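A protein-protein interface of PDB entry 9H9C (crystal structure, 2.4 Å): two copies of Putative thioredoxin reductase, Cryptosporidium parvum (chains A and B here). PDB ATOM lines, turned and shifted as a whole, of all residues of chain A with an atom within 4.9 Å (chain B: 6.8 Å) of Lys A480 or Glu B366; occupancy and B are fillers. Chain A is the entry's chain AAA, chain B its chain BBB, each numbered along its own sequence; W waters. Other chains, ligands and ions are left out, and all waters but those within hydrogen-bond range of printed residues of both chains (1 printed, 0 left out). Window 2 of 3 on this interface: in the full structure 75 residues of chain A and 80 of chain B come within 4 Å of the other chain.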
ATOM      1  N   THR A 478      11.124   2.062 -33.871  1.00  0.00           N
ATOM      2  CA  THR A 478      11.949   1.279 -32.924  1.00  0.00           C
ATOM      3  C   THR A 478      11.097   0.817 -31.732  1.00  0.00           C
ATOM      4  O   THR A 478      10.027   1.412 -31.482  1.00  0.00           O
ATOM      5  CB  THR A 478      13.127   2.122 -32.421  1.00  0.00           C
ATOM      6  OG1 THR A 478      12.565   3.201 -31.669  1.00  0.00           O
ATOM      7  CG2 THR A 478      14.007   2.609 -33.553  1.00  0.00           C
ATOM      8  N   LYS A 479      11.598  -0.135 -30.962  1.00  0.00           N
ATOM      9  CA  LYS A 479      10.973  -0.523 -29.680  1.00  0.00           C
ATOM     10  C   LYS A 479      10.734   0.720 -28.796  1.00  0.00           C
ATOM     11  O   LYS A 479       9.697   0.767 -28.144  1.00  0.00           O
ATOM     12  CB  LYS A 479      11.785  -1.599 -28.954  1.00  0.00           C
ATOM     13  CG  LYS A 479      11.122  -2.114 -27.686  1.00  0.00           C
ATOM     14  CD  LYS A 479       9.686  -2.511 -27.886  1.00  0.00           C
ATOM     15  CE  LYS A 479       9.144  -3.435 -26.809  1.00  0.00           C
ATOM     16  NZ  LYS A 479       9.244  -2.806 -25.472  1.00  0.00           N
ATOM     17  N   LYS A 480      11.628   1.702 -28.809  1.00  0.00           N
ATOM     18  CA  LYS A 480      11.532   2.935 -27.977  1.00  0.00           C
ATOM     19  C   LYS A 480      10.280   3.705 -28.436  1.00  0.00           C
ATOM     20  O   LYS A 480       9.494   4.131 -27.569  1.00  0.00           O
ATOM     21  CB  LYS A 480      12.823   3.763 -28.052  1.00  0.00           C
ATOM     22  CG  LYS A 480      12.746   5.144 -27.431  1.00  0.00           C
ATOM     23  CD  LYS A 480      14.116   5.742 -27.121  1.00  0.00           C
ATOM     24  CE  LYS A 480      14.066   7.196 -26.653  1.00  0.00           C
ATOM     25  NZ  LYS A 480      12.989   7.471 -25.638  1.00  0.00           N
ATOM     26  N   ASP A 481      10.104   3.839 -29.756  1.00  0.00           N
ATOM     27  CA  ASP A 481       8.950   4.525 -30.372  1.00  0.00           C
ATOM     28  C   ASP A 481       7.655   3.878 -29.862  1.00  0.00           C
ATOM     29  O   ASP A 481       6.696   4.622 -29.557  1.00  0.00           O
ATOM     30  CB  ASP A 481       9.016   4.469 -31.897  1.00  0.00           C
ATOM     31  CG  ASP A 481      10.191   5.262 -32.462  1.00  0.00           C
ATOM     32  OD1 ASP A 481      10.621   6.277 -31.797  1.00  0.00           O
ATOM     33  OD2 ASP A 481      10.718   4.844 -33.526  1.00  0.00           O
ATOM     34  N   PHE A 482       7.632   2.546 -29.797  1.00  0.00           N
ATOM     35  CA  PHE A 482       6.470   1.753 -29.348  1.00  0.00           C
ATOM     36  C   PHE A 482       6.214   2.027 -27.853  1.00  0.00           C
ATOM     37  O   PHE A 482       5.054   2.217 -27.492  1.00  0.00           O
ATOM     38  CB  PHE A 482       6.697   0.268 -29.658  1.00  0.00           C
ATOM     39  CG  PHE A 482       6.262  -0.172 -31.030  1.00  0.00           C
ATOM     40  CD1 PHE A 482       7.050   0.052 -32.140  1.00  0.00           C
ATOM     41  CD2 PHE A 482       5.043  -0.799 -31.214  1.00  0.00           C
ATOM     42  CE1 PHE A 482       6.629  -0.331 -33.406  1.00  0.00           C
ATOM     43  CE2 PHE A 482       4.606  -1.177 -32.473  1.00  0.00           C
ATOM     44  CZ  PHE A 482       5.413  -0.959 -33.571  1.00  0.00           C
ATOM     45  N   ASP A 483       7.250   2.076 -27.019  1.00  0.00           N
ATOM     46  CA  ASP A 483       7.121   2.273 -25.564  1.00  0.00           C
ATOM     47  C   ASP A 483       6.660   3.694 -25.253  1.00  0.00           C
ATOM     48  O   ASP A 483       5.996   3.876 -24.211  1.00  0.00           O
ATOM     49  CB  ASP A 483       8.427   2.026 -24.816  1.00  0.00           C
ATOM     50  CG  ASP A 483       8.881   0.582 -24.809  1.00  0.00           C
ATOM     51  OD1 ASP A 483       8.053  -0.302 -25.112  1.00  0.00           O
ATOM     52  OD2 ASP A 483      10.077   0.354 -24.519  1.00  0.00           O
ATOM     53  N   ASP A 484       7.033   4.682 -26.064  1.00  0.00           N
ATOM     54  CA  ASP A 484       6.724   6.115 -25.807  1.00  0.00           C
ATOM     55  C   ASP A 484       5.402   6.487 -26.492  1.00  0.00           C
ATOM     56  O   ASP A 484       5.005   7.635 -26.338  1.00  0.00           O
ATOM     57  CB  ASP A 484       7.864   7.038 -26.242  1.00  0.00           C
ATOM     58  CG  ASP A 484       9.212   6.799 -25.570  1.00  0.00           C
ATOM     59  OD1 ASP A 484       9.304   5.950 -24.682  1.00  0.00           O
ATOM     60  OD2 ASP A 484      10.196   7.450 -25.978  1.00  0.00           O
ATOM     61  N   ASP B 325       4.551  18.074 -13.731  1.00  0.00           N
ATOM     62  CA  ASP B 325       4.210  17.157 -12.605  1.00  0.00           C
ATOM     63  C   ASP B 325       4.614  17.780 -11.247  1.00  0.00           C
ATOM     64  O   ASP B 325       4.006  17.393 -10.234  1.00  0.00           O
ATOM     65  CB  ASP B 325       4.794  15.759 -12.818  1.00  0.00           C
ATOM     66  CG  ASP B 325       4.496  15.131 -14.194  1.00  0.00           C
ATOM     67  OD1 ASP B 325       3.502  15.495 -14.877  1.00  0.00           O
ATOM     68  OD2 ASP B 325       5.256  14.264 -14.588  1.00  0.00           O
ATOM     69  N   LYS B 351       1.199   6.838 -17.843  1.00  0.00           N
ATOM     70  CA  LYS B 351       2.563   7.085 -18.353  1.00  0.00           C
ATOM     71  C   LYS B 351       3.178   8.235 -17.541  1.00  0.00           C
ATOM     72  O   LYS B 351       4.377   8.211 -17.278  1.00  0.00           O
ATOM     73  CB  LYS B 351       2.598   7.358 -19.860  1.00  0.00           C
ATOM     74  CG  LYS B 351       4.017   7.477 -20.382  1.00  0.00           C
ATOM     75  CD  LYS B 351       4.160   7.475 -21.897  1.00  0.00           C
ATOM     76  CE  LYS B 351       3.882   6.137 -22.591  1.00  0.00           C
ATOM     77  NZ  LYS B 351       4.850   5.054 -22.255  1.00  0.00           N
ATOM     78  N   LEU B 355       6.731   7.749 -15.738  1.00  0.00           N
ATOM     79  CA  LEU B 355       7.870   8.618 -16.109  1.00  0.00           C
ATOM     80  C   LEU B 355       8.294   9.440 -14.876  1.00  0.00           C
ATOM     81  O   LEU B 355       9.525   9.603 -14.676  1.00  0.00           O
ATOM     82  CB  LEU B 355       7.482   9.492 -17.295  1.00  0.00           C
ATOM     83  CG  LEU B 355       7.284   8.779 -18.642  1.00  0.00           C
ATOM     84  CD1 LEU B 355       7.124   9.828 -19.728  1.00  0.00           C
ATOM     85  CD2 LEU B 355       8.422   7.841 -19.003  1.00  0.00           C
ATOM     86  N   LEU B 356       7.339   9.906 -14.062  1.00  0.00           N
ATOM     87  CA  LEU B 356       7.640  10.645 -12.808  1.00  0.00           C
ATOM     88  C   LEU B 356       8.489   9.737 -11.912  1.00  0.00           C
ATOM     89  O   LEU B 356       9.606  10.148 -11.558  1.00  0.00           O
ATOM     90  CB  LEU B 356       6.347  11.074 -12.107  1.00  0.00           C
ATOM     91  CG  LEU B 356       6.494  11.651 -10.696  1.00  0.00           C
ATOM     92  CD1 LEU B 356       7.302  12.945 -10.674  1.00  0.00           C
ATOM     93  CD2 LEU B 356       5.144  11.889 -10.059  1.00  0.00           C
ATOM     94  N   ARG B 358      10.361   7.264 -12.625  1.00  0.00           N
ATOM     95  CA  ARG B 358      11.720   7.101 -13.229  1.00  0.00           C
ATOM     96  C   ARG B 358      12.575   8.360 -13.048  1.00  0.00           C
ATOM     97  O   ARG B 358      13.755   8.218 -12.750  1.00  0.00           O
ATOM     98  CB  ARG B 358      11.621   6.745 -14.716  1.00  0.00           C
ATOM     99  CG  ARG B 358      11.150   5.320 -14.960  1.00  0.00           C
ATOM    100  CD  ARG B 358      10.946   4.984 -16.422  1.00  0.00           C
ATOM    101  NE  ARG B 358      10.292   3.679 -16.537  1.00  0.00           N
ATOM    102  CZ  ARG B 358       9.735   3.234 -17.653  1.00  0.00           C
ATOM    103  NH1 ARG B 358       9.765   3.983 -18.746  1.00  0.00           N
ATOM    104  NH2 ARG B 358       9.144   2.053 -17.676  1.00  0.00           N
ATOM    105  N   ARG B 359      12.013   9.550 -13.278  1.00  0.00           N
ATOM    106  CA  ARG B 359      12.751  10.833 -13.140  1.00  0.00           C
ATOM    107  C   ARG B 359      13.224  11.001 -11.685  1.00  0.00           C
ATOM    108  O   ARG B 359      14.347  11.515 -11.473  1.00  0.00           O
ATOM    109  CB  ARG B 359      11.898  12.021 -13.592  1.00  0.00           C
ATOM    110  CG  ARG B 359      11.637  12.080 -15.090  1.00  0.00           C
ATOM    111  CD  ARG B 359      11.247  13.454 -15.591  1.00  0.00           C
ATOM    112  NE  ARG B 359      10.140  14.001 -14.837  1.00  0.00           N
ATOM    113  CZ  ARG B 359       8.872  13.676 -15.003  1.00  0.00           C
ATOM    114  NH1 ARG B 359       8.521  12.793 -15.921  1.00  0.00           N
ATOM    115  NH2 ARG B 359       7.964  14.216 -14.204  1.00  0.00           N
ATOM    116  N   GLY B 363      17.067   8.504 -12.647  1.00  0.00           N
ATOM    117  CA  GLY B 363      17.844   9.493 -13.414  1.00  0.00           C
ATOM    118  C   GLY B 363      17.312   9.730 -14.815  1.00  0.00           C
ATOM    119  O   GLY B 363      18.105  10.210 -15.665  1.00  0.00           O
ATOM    120  N   SER B 364      16.032   9.435 -15.064  1.00  0.00           N
ATOM    121  CA  SER B 364      15.335   9.710 -16.346  1.00  0.00           C
ATOM    122  C   SER B 364      15.017  11.211 -16.425  1.00  0.00           C
ATOM    123  O   SER B 364      14.924  11.861 -15.363  1.00  0.00           O
ATOM    124  CB  SER B 364      14.092   8.831 -16.501  1.00  0.00           C
ATOM    125  OG  SER B 364      13.233   9.291 -17.542  1.00  0.00           O
ATOM    126  N   ASN B 365      14.912  11.765 -17.630  1.00  0.00           N
ATOM    127  CA  ASN B 365      14.414  13.143 -17.841  1.00  0.00           C
ATOM    128  C   ASN B 365      13.349  13.128 -18.948  1.00  0.00           C
ATOM    129  O   ASN B 365      13.159  14.163 -19.630  1.00  0.00           O
ATOM    130  CB  ASN B 365      15.556  14.124 -18.120  1.00  0.00           C
ATOM    131  CG  ASN B 365      16.341  13.836 -19.385  1.00  0.00           C
ATOM    132  OD1 ASN B 365      15.899  13.104 -20.276  1.00  0.00           O
ATOM    133  ND2 ASN B 365      17.524  14.419 -19.478  1.00  0.00           N
ATOM    134  N   GLU B 366      12.639  12.003 -19.097  1.00  0.00           N
ATOM    135  CA  GLU B 366      11.641  11.787 -20.176  1.00  0.00           C
ATOM    136  C   GLU B 366      10.282  12.219 -19.643  1.00  0.00           C
ATOM    137  O   GLU B 366       9.913  11.820 -18.516  1.00  0.00           O
ATOM    138  CB  GLU B 366      11.643  10.340 -20.691  1.00  0.00           C
ATOM    139  CG  GLU B 366      12.903   9.986 -21.503  1.00  0.00           C
ATOM    140  CD  GLU B 366      12.781   9.324 -22.873  1.00  0.00           C
ATOM    141  OE1 GLU B 366      12.460   8.105 -22.934  1.00  0.00           O
ATOM    142  OE2 GLU B 366      13.019  10.042 -23.887  1.00  0.00           O
ATOM    143  N   PHE B 367       9.618  13.068 -20.432  1.00  0.00           N
ATOM    144  CA  PHE B 367       8.230  13.534 -20.248  1.00  0.00           C
ATOM    145  C   PHE B 367       7.391  12.995 -21.414  1.00  0.00           C
ATOM    146  O   PHE B 367       7.954  12.597 -22.448  1.00  0.00           O
ATOM    147  CB  PHE B 367       8.197  15.064 -20.140  1.00  0.00           C
ATOM    148  CG  PHE B 367       8.812  15.612 -18.880  1.00  0.00           C
ATOM    149  CD1 PHE B 367      10.190  15.783 -18.801  1.00  0.00           C
ATOM    150  CD2 PHE B 367       8.022  15.948 -17.770  1.00  0.00           C
ATOM    151  CE1 PHE B 367      10.778  16.273 -17.642  1.00  0.00           C
ATOM    152  CE2 PHE B 367       8.612  16.443 -16.606  1.00  0.00           C
ATOM    153  CZ  PHE B 367       9.991  16.592 -16.540  1.00  0.00           C
ATOM    154  N   ILE B 368       6.060  12.979 -21.250  1.00  0.00           N
ATOM    155  CA  ILE B 368       5.115  12.747 -22.383  1.00  0.00           C
ATOM    156  C   ILE B 368       5.273  13.886 -23.398  1.00  0.00           C
ATOM    157  O   ILE B 368       5.515  15.061 -22.979  1.00  0.00           O
ATOM    158  CB  ILE B 368       3.666  12.643 -21.879  1.00  0.00           C
ATOM    159  CG1 ILE B 368       3.441  11.370 -21.064  1.00  0.00           C
ATOM    160  CG2 ILE B 368       2.689  12.735 -23.033  1.00  0.00           C
ATOM    161  CD1 ILE B 368       2.250  11.443 -20.131  1.00  0.00           C
ATOM    162  N   LYS B 474       3.072  10.282 -35.431  1.00  0.00           N
ATOM    163  CA  LYS B 474       4.089  10.815 -34.480  1.00  0.00           C
ATOM    164  C   LYS B 474       5.496  10.734 -35.103  1.00  0.00           C
ATOM    165  O   LYS B 474       6.293  11.679 -34.873  1.00  0.00           O
ATOM    166  CB  LYS B 474       3.996  10.060 -33.151  1.00  0.00           C
ATOM    167  CG  LYS B 474       4.960  10.547 -32.086  1.00  0.00           C
ATOM    168  CD  LYS B 474       4.874   9.803 -30.806  1.00  0.00           C
ATOM    169  CE  LYS B 474       5.653  10.472 -29.697  1.00  0.00           C
ATOM    170  NZ  LYS B 474       5.719   9.581 -28.508  1.00  0.00           N
HETATM  171  O   HOH W   1       6.445   7.028 -29.563  1.00  0.00           O
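Water W1 bridges O of Asp A481 and NZ of Lys B474.
The backbone carbonyl oxygen (O) of Asp A483 lies within hydrogen-bond range of the side-chain amino group (NZ) of Lys B351, 2.6 Å away. The backbone carbonyl oxygen (O) of Asp A484 is in hydrogen-bond range of the side-chain amino group (NZ) of Lys B474 (3.0 Å). OE1 of Glu B366 lies within salt-bridge range of NZ of Lys A480 (2.8 Å).
Lys A480 touches one residue of chain B. Of the printed residues of chain B, Asp A484 touches Glu B366 (3.8 Å) and Lys B474 (3.0 Å). Of the printed residues of chain A, Lys B474 touches Asp A484 (3.0 Å). The nearest printed residue of chain A that does not touch Glu B366 is Asp A483 (7.5 Å).
No position is printed for both chains. Of the 4 pairs that touch across the chains among the printed residues, none has its exchanged pair printed and touching as well.
OD2 of Asp A484 lies within salt-bridge range of NZ of Lys A480. NH1 of Arg B359 is in hydrogen-bond range of O of Glu B366 (3.1 Å). OG of Ser B364 is in hydrogen-bond range of N of Glu B366, 3.2 Å away. OG1 of Thr A478 sits close to N of Lys A480. The side-chain carboxylate (OD1) of Asp A483 is in salt-bridge range of the side-chain amino group (NZ) of Lys A479 (2.8 Å).
Of the 13 printed residues of chain B, 3 touch a printed residue of chain A. Printed residues of chain B that touch a printed residue of chain A: Lys B351, Glu B366 and Lys B474. Among the printed residues, 4 pairs touch across the chains. Among the printed residues, Asp or Glu carboxylates within 4 Å of a Lys or Arg side-chain nitrogen of the other chain: Lys A480 with Glu B366.
Among the printed residues, pairs that only touch across the chains: Asp A484 with Glu B366.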
